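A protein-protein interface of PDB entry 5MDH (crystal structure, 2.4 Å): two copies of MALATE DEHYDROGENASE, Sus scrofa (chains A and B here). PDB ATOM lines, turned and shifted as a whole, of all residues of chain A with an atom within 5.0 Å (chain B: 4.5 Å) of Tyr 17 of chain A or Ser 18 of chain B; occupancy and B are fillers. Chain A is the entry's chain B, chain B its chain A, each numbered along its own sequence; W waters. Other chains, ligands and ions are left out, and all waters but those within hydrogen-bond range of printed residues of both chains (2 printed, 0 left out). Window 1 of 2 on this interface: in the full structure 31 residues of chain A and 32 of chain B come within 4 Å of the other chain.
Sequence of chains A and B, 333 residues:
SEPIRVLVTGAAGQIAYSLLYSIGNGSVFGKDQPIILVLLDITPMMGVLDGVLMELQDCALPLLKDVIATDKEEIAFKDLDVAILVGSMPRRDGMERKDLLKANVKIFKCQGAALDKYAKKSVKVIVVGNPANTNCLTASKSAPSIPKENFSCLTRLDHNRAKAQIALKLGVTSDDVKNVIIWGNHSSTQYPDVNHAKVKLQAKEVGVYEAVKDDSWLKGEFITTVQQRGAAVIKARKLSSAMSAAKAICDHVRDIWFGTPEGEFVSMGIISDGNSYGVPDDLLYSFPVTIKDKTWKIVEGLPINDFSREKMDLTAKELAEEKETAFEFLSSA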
ATOM      1  N   GLY A  13       3.293   2.936  17.849  1.00  0.00           N
ATOM      2  CA  GLY A  13       2.338   3.349  18.848  1.00  0.00           C
ATOM      3  C   GLY A  13       0.860   3.412  18.917  1.00  0.00           C
ATOM      4  O   GLY A  13       0.289   4.270  18.262  1.00  0.00           O
ATOM      5  N   GLN A  14       0.051   2.557  19.535  1.00  0.00           N
ATOM      6  CA  GLN A  14      -1.402   2.687  19.652  1.00  0.00           C
ATOM      7  C   GLN A  14      -2.208   2.506  18.372  1.00  0.00           C
ATOM      8  O   GLN A  14      -2.683   1.401  18.126  1.00  0.00           O
ATOM      9  CB  GLN A  14      -1.679   4.091  20.176  1.00  0.00           C
ATOM     10  CG  GLN A  14      -2.680   4.229  21.297  1.00  0.00           C
ATOM     11  CD  GLN A  14      -1.960   4.362  22.626  1.00  0.00           C
ATOM     12  OE1 GLN A  14      -0.791   4.027  22.702  1.00  0.00           O
ATOM     13  NE2 GLN A  14      -2.684   4.805  23.647  1.00  0.00           N
ATOM     14  N   ILE A  15      -2.383   3.531  17.562  1.00  0.00           N
ATOM     15  CA  ILE A  15      -3.140   3.497  16.329  1.00  0.00           C
ATOM     16  C   ILE A  15      -2.626   2.487  15.324  1.00  0.00           C
ATOM     17  O   ILE A  15      -3.390   1.626  14.864  1.00  0.00           O
ATOM     18  CB  ILE A  15      -3.283   4.900  15.703  1.00  0.00           C
ATOM     19  CG1 ILE A  15      -4.144   5.743  16.668  1.00  0.00           C
ATOM     20  CG2 ILE A  15      -3.916   4.891  14.318  1.00  0.00           C
ATOM     21  CD1 ILE A  15      -4.264   7.172  16.185  1.00  0.00           C
ATOM     22  N   ALA A  16      -1.328   2.499  15.077  1.00  0.00           N
ATOM     23  CA  ALA A  16      -0.678   1.535  14.194  1.00  0.00           C
ATOM     24  C   ALA A  16      -0.772   0.119  14.732  1.00  0.00           C
ATOM     25  O   ALA A  16      -0.978  -0.855  13.990  1.00  0.00           O
ATOM     26  CB  ALA A  16       0.794   1.932  13.998  1.00  0.00           C
ATOM     27  N   TYR A  17      -0.688  -0.042  16.048  1.00  0.00           N
ATOM     28  CA  TYR A  17      -0.751  -1.383  16.655  1.00  0.00           C
ATOM     29  C   TYR A  17      -2.151  -1.943  16.414  1.00  0.00           C
ATOM     30  O   TYR A  17      -2.236  -3.132  16.124  1.00  0.00           O
ATOM     31  CB  TYR A  17      -0.395  -1.391  18.132  1.00  0.00           C
ATOM     32  CG  TYR A  17      -0.123  -2.741  18.747  1.00  0.00           C
ATOM     33  CD1 TYR A  17       1.065  -3.410  18.424  1.00  0.00           C
ATOM     34  CD2 TYR A  17      -0.995  -3.355  19.640  1.00  0.00           C
ATOM     35  CE1 TYR A  17       1.362  -4.642  18.963  1.00  0.00           C
ATOM     36  CE2 TYR A  17      -0.713  -4.584  20.198  1.00  0.00           C
ATOM     37  CZ  TYR A  17       0.469  -5.223  19.850  1.00  0.00           C
ATOM     38  OH  TYR A  17       0.762  -6.485  20.379  1.00  0.00           O
ATOM     39  N   SER A  18      -3.184  -1.086  16.455  1.00  0.00           N
ATOM     40  CA  SER A  18      -4.523  -1.595  16.151  1.00  0.00           C
ATOM     41  C   SER A  18      -4.784  -1.753  14.660  1.00  0.00           C
ATOM     42  O   SER A  18      -5.717  -2.452  14.267  1.00  0.00           O
ATOM     43  CB  SER A  18      -5.578  -0.671  16.753  1.00  0.00           C
ATOM     44  OG  SER A  18      -5.761  -0.936  18.148  1.00  0.00           O
ATOM     45  N   LEU A  19      -4.033  -1.063  13.797  1.00  0.00           N
ATOM     46  CA  LEU A  19      -4.226  -1.031  12.380  1.00  0.00           C
ATOM     47  C   LEU A  19      -3.421  -1.967  11.493  1.00  0.00           C
ATOM     48  O   LEU A  19      -3.988  -2.362  10.470  1.00  0.00           O
ATOM     49  CB  LEU A  19      -3.921   0.413  11.915  1.00  0.00           C
ATOM     50  CG  LEU A  19      -3.672   0.629  10.432  1.00  0.00           C
ATOM     51  CD1 LEU A  19      -4.973   0.503   9.629  1.00  0.00           C
ATOM     52  CD2 LEU A  19      -2.969   1.951  10.118  1.00  0.00           C
ATOM     53  N   LEU A  20      -2.185  -2.324  11.811  1.00  0.00           N
ATOM     54  CA  LEU A  20      -1.394  -3.156  10.918  1.00  0.00           C
ATOM     55  C   LEU A  20      -1.929  -4.532  10.599  1.00  0.00           C
ATOM     56  O   LEU A  20      -1.762  -4.900   9.427  1.00  0.00           O
ATOM     57  CB  LEU A  20       0.056  -3.205  11.448  1.00  0.00           C
ATOM     58  CG  LEU A  20       0.686  -1.809  11.549  1.00  0.00           C
ATOM     59  CD1 LEU A  20       1.898  -1.808  12.476  1.00  0.00           C
ATOM     60  CD2 LEU A  20       1.040  -1.284  10.173  1.00  0.00           C
ATOM     61  N   VAL A  52       7.038  -5.261  17.084  1.00  0.00           N
ATOM     62  CA  VAL A  52       5.809  -5.157  16.306  1.00  0.00           C
ATOM     63  C   VAL A  52       6.021  -5.941  15.014  1.00  0.00           C
ATOM     64  O   VAL A  52       5.123  -6.600  14.519  1.00  0.00           O
ATOM     65  CB  VAL A  52       5.473  -3.681  15.985  1.00  0.00           C
ATOM     66  CG1 VAL A  52       4.437  -3.525  14.890  1.00  0.00           C
ATOM     67  CG2 VAL A  52       5.036  -2.969  17.269  1.00  0.00           C
ATOM     68  N   GLU A  55       5.746  -9.417  15.826  1.00  0.00           N
ATOM     69  CA  GLU A  55       4.329  -9.803  15.946  1.00  0.00           C
ATOM     70  C   GLU A  55       3.654  -9.997  14.598  1.00  0.00           C
ATOM     71  O   GLU A  55       2.885 -10.943  14.396  1.00  0.00           O
ATOM     72  CB  GLU A  55       3.479  -8.861  16.818  1.00  0.00           C
ATOM     73  CG  GLU A  55       3.896  -8.977  18.279  1.00  0.00           C
ATOM     74  CD  GLU A  55       2.786  -8.644  19.258  1.00  0.00           C
ATOM     75  OE1 GLU A  55       1.811  -9.441  19.263  1.00  0.00           O
ATOM     76  OE2 GLU A  55       2.873  -7.633  19.991  1.00  0.00           O
ATOM     77  N   GLN B  14      -4.617  -5.514  26.986  1.00  0.00           N
ATOM     78  CA  GLN B  14      -4.066  -5.520  25.648  1.00  0.00           C
ATOM     79  C   GLN B  14      -4.549  -6.577  24.658  1.00  0.00           C
ATOM     80  O   GLN B  14      -4.880  -6.214  23.505  1.00  0.00           O
ATOM     81  CB  GLN B  14      -2.539  -5.658  25.765  1.00  0.00           C
ATOM     82  CG  GLN B  14      -1.819  -4.877  24.702  1.00  0.00           C
ATOM     83  CD  GLN B  14      -0.321  -5.184  24.676  1.00  0.00           C
ATOM     84  OE1 GLN B  14       0.232  -6.024  25.410  1.00  0.00           O
ATOM     85  NE2 GLN B  14       0.295  -4.448  23.757  1.00  0.00           N
ATOM     86  N   ILE B  15      -4.473  -7.848  25.001  1.00  0.00           N
ATOM     87  CA  ILE B  15      -4.910  -8.967  24.172  1.00  0.00           C
ATOM     88  C   ILE B  15      -6.369  -8.782  23.786  1.00  0.00           C
ATOM     89  O   ILE B  15      -6.719  -8.809  22.604  1.00  0.00           O
ATOM     90  CB  ILE B  15      -4.770 -10.272  24.983  1.00  0.00           C
ATOM     91  CG1 ILE B  15      -3.288 -10.489  25.278  1.00  0.00           C
ATOM     92  CG2 ILE B  15      -5.390 -11.490  24.300  1.00  0.00           C
ATOM     93  CD1 ILE B  15      -3.030 -11.682  26.178  1.00  0.00           C
ATOM     94  N   ALA B  16      -7.260  -8.583  24.751  1.00  0.00           N
ATOM     95  CA  ALA B  16      -8.666  -8.294  24.493  1.00  0.00           C
ATOM     96  C   ALA B  16      -8.775  -7.065  23.586  1.00  0.00           C
ATOM     97  O   ALA B  16      -9.450  -7.174  22.537  1.00  0.00           O
ATOM     98  CB  ALA B  16      -9.515  -8.038  25.719  1.00  0.00           C
ATOM     99  N   TYR B  17      -8.061  -5.975  23.859  1.00  0.00           N
ATOM    100  CA  TYR B  17      -8.118  -4.827  22.952  1.00  0.00           C
ATOM    101  C   TYR B  17      -7.799  -5.170  21.502  1.00  0.00           C
ATOM    102  O   TYR B  17      -8.358  -4.508  20.600  1.00  0.00           O
ATOM    103  CB  TYR B  17      -7.208  -3.667  23.387  1.00  0.00           C
ATOM    104  CG  TYR B  17      -7.585  -2.344  22.755  1.00  0.00           C
ATOM    105  CD1 TYR B  17      -8.782  -1.711  23.058  1.00  0.00           C
ATOM    106  CD2 TYR B  17      -6.718  -1.735  21.846  1.00  0.00           C
ATOM    107  CE1 TYR B  17      -9.122  -0.485  22.463  1.00  0.00           C
ATOM    108  CE2 TYR B  17      -7.063  -0.534  21.257  1.00  0.00           C
ATOM    109  CZ  TYR B  17      -8.234   0.098  21.562  1.00  0.00           C
ATOM    110  OH  TYR B  17      -8.508   1.319  20.966  1.00  0.00           O
ATOM    111  N   SER B  18      -6.965  -6.186  21.267  1.00  0.00           N
ATOM    112  CA  SER B  18      -6.593  -6.611  19.935  1.00  0.00           C
ATOM    113  C   SER B  18      -7.529  -7.671  19.369  1.00  0.00           C
ATOM    114  O   SER B  18      -7.322  -8.080  18.224  1.00  0.00           O
ATOM    115  CB  SER B  18      -5.197  -7.275  19.941  1.00  0.00           C
ATOM    116  OG  SER B  18      -4.128  -6.361  20.161  1.00  0.00           O
ATOM    117  N   LEU B  19      -8.481  -8.158  20.121  1.00  0.00           N
ATOM    118  CA  LEU B  19      -9.351  -9.268  19.811  1.00  0.00           C
ATOM    119  C   LEU B  19     -10.841  -8.960  19.714  1.00  0.00           C
ATOM    120  O   LEU B  19     -11.512  -9.606  18.902  1.00  0.00           O
ATOM    121  CB  LEU B  19      -9.138 -10.325  20.932  1.00  0.00           C
ATOM    122  CG  LEU B  19     -10.053 -11.555  20.967  1.00  0.00           C
ATOM    123  CD1 LEU B  19      -9.859 -12.447  19.737  1.00  0.00           C
ATOM    124  CD2 LEU B  19      -9.898 -12.347  22.265  1.00  0.00           C
ATOM    125  N   LEU B  20     -11.396  -8.032  20.479  1.00  0.00           N
ATOM    126  CA  LEU B  20     -12.850  -7.825  20.416  1.00  0.00           C
ATOM    127  C   LEU B  20     -13.327  -7.462  19.024  1.00  0.00           C
ATOM    128  O   LEU B  20     -14.399  -7.974  18.653  1.00  0.00           O
ATOM    129  CB  LEU B  20     -13.376  -6.869  21.499  1.00  0.00           C
ATOM    130  CG  LEU B  20     -12.772  -7.138  22.878  1.00  0.00           C
ATOM    131  CD1 LEU B  20     -13.303  -6.223  23.984  1.00  0.00           C
ATOM    132  CD2 LEU B  20     -12.929  -8.604  23.238  1.00  0.00           C
ATOM    133  N   ARG B 237       9.256  -5.124  22.776  1.00  0.00           N
ATOM    134  CA  ARG B 237       8.111  -4.295  23.068  1.00  0.00           C
ATOM    135  C   ARG B 237       8.055  -3.803  24.511  1.00  0.00           C
ATOM    136  O   ARG B 237       7.595  -2.670  24.675  1.00  0.00           O
ATOM    137  CB  ARG B 237       6.792  -4.999  22.720  1.00  0.00           C
ATOM    138  CG  ARG B 237       6.720  -5.474  21.277  1.00  0.00           C
ATOM    139  CD  ARG B 237       5.361  -5.188  20.669  1.00  0.00           C
ATOM    140  NE  ARG B 237       4.274  -5.526  21.581  1.00  0.00           N
ATOM    141  CZ  ARG B 237       3.343  -4.632  21.945  1.00  0.00           C
ATOM    142  NH1 ARG B 237       3.444  -3.405  21.472  1.00  0.00           N
ATOM    143  NH2 ARG B 237       2.368  -4.961  22.761  1.00  0.00           N
ATOM    144  N   SER B 241       3.057 -10.131  23.915  1.00  0.00           N
ATOM    145  CA  SER B 241       2.540 -10.070  22.532  1.00  0.00           C
ATOM    146  C   SER B 241       1.045  -9.867  22.712  1.00  0.00           C
ATOM    147  O   SER B 241       0.582 -10.314  23.783  1.00  0.00           O
ATOM    148  CB  SER B 241       2.892 -11.394  21.866  1.00  0.00           C
ATOM    149  OG  SER B 241       1.848 -12.327  22.128  1.00  0.00           O
ATOM    150  N   ALA B 242       0.304  -9.286  21.801  1.00  0.00           N
ATOM    151  CA  ALA B 242      -1.128  -9.086  21.965  1.00  0.00           C
ATOM    152  C   ALA B 242      -1.803  -9.186  20.597  1.00  0.00           C
ATOM    153  O   ALA B 242      -2.776  -9.892  20.345  1.00  0.00           O
ATOM    154  CB  ALA B 242      -1.403  -7.760  22.662  1.00  0.00           C
ATOM    155  N   MET B 243      -1.226  -8.464  19.636  1.00  0.00           N
ATOM    156  CA  MET B 243      -1.720  -8.498  18.270  1.00  0.00           C
ATOM    157  C   MET B 243      -1.656  -9.899  17.697  1.00  0.00           C
ATOM    158  O   MET B 243      -2.603 -10.374  17.096  1.00  0.00           O
ATOM    159  CB  MET B 243      -0.870  -7.558  17.384  1.00  0.00           C
ATOM    160  CG  MET B 243      -1.315  -7.523  15.930  1.00  0.00           C
ATOM    161  SD  MET B 243      -0.124  -6.802  14.824  1.00  0.00           S
ATOM    162  CE  MET B 243       0.860  -8.124  14.292  1.00  0.00           C
ATOM    163  N   ALA B 246      -3.939 -12.407  20.043  1.00  0.00           N
ATOM    164  CA  ALA B 246      -5.335 -12.281  19.637  1.00  0.00           C
ATOM    165  C   ALA B 246      -5.717 -12.992  18.333  1.00  0.00           C
ATOM    166  O   ALA B 246      -6.814 -13.528  18.152  1.00  0.00           O
ATOM    167  CB  ALA B 246      -5.623 -10.786  19.428  1.00  0.00           C
HETATM  168  O   HOH W   1      -3.781  -5.044  17.733  1.00  0.00           O
HETATM  169  O   HOH W   2      -7.677  -3.068  18.507  1.00  0.00           O
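N of Ala 242 of chain B is in hydrogen-bond range of OE1 of Glu 55 of chain A (3.0 Å). NE of Arg 237 of chain B lies within salt-bridge range of OE2 of Glu 55 of chain A. The side-chain carboxylate of Glu 55 of chain A sits at hydrogen-bond distance from the backbone NH of Met 243 of chain B (3.2 Å). N of Ala 242 of chain B sits at hydrogen-bond distance from OH of Tyr 17 of chain A, at 3.2 Å. The side-chain hydroxyl of Tyr 17 of chain A is in hydrogen-bond range of the guanidinium group of Arg 237 of chain B (3.3 Å). N of Met 243 of chain B lies within hydrogen-bond range of OH of Tyr 17 of chain A.
OE2 of Glu 55 of chain A is in hydrogen-bond range of OH of Tyr 17 of chain A, 2.4 Å away. The backbone carbonyl oxygen (O) of Gln 14 of chain B lies within hydrogen-bond range of the side-chain hydroxyl (OG) of Ser 18 of chain B.
Gln 14 of chain B touches Tyr 17 of chain A (NE2 to CE2, 3.7 Å). Tyr 17 of chain A touches Ser 18 of chain B. Ser 18 of chain A touches Tyr 17 of chain B. Arg 237 of chain B touches Val 52 of chain A (CD to N, 3.96 Å). Glu 55 of chain A touches Ser 241 of chain B.
Of the printed residues of chain B, Tyr 17 of chain A touches Gln 14 (3.7 Å), Ser 18 (3.8 Å), Arg 237 (3.3 Å), Ala 242 (3.2 Å) and Met 243 (2.9 Å). Printed residues of chain B within 4 Å of Ser 18 of chain A: Tyr 17. Of the printed residues of chain A, Gln 14 of chain B touches Tyr 17 (3.7 Å). Of chain A, only Tyr 17 comes within 4 Å of Ser 18 of chain B. The nearest residue of chain B that does not touch Tyr 17 of chain A is Ser 241 of chain B (4.1 Å). The nearest printed residue of chain A that does not touch Ser 18 of chain B is Ser 18 of chain A (6.0 Å). The nearest printed residue of chain A that does not touch Met 243 of chain B is Val 52 of chain A (4.5 Å).
Printed residues of chain B that touch a printed residue of chain A: Gln 14, Tyr 17, Ser 18, Arg 237, Ser 241, Ala 242 and Met 243. Hydrophobic or aromatic side chains of chain A within 4 Å of the printed part of chain B: Tyr 17.
Tyr 17 of chain A touches Gln 14 of chain B, but with the chains exchanged Gln 14 of chain A does not touch Tyr 17 of chain B (5.7 Å). Tyr 17 of chain A touches Ser 18 of chain B, and with the chains exchanged Ser 18 of chain A touches Tyr 17 of chain B. Positions printed for both chains: 14, 15, 16, 17, 18, 19 and 20. Of the 11 pairs that touch across the chains among the printed residues, 2 have their exchanged pair printed and touching as well.
Water W2 lies within hydrogen-bond range of the backbone carbonyl oxygen of Tyr 17 of chain B (2.6 Å) and the side-chain hydroxyl of Ser 18 of chain A (2.9 Å). Water W1 bridges the side-chain hydroxyl (OG) of Ser 18 of chain B (2.8 Å) and the backbone carbonyl oxygen (O) of Tyr 17 of chain A (2.9 Å).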
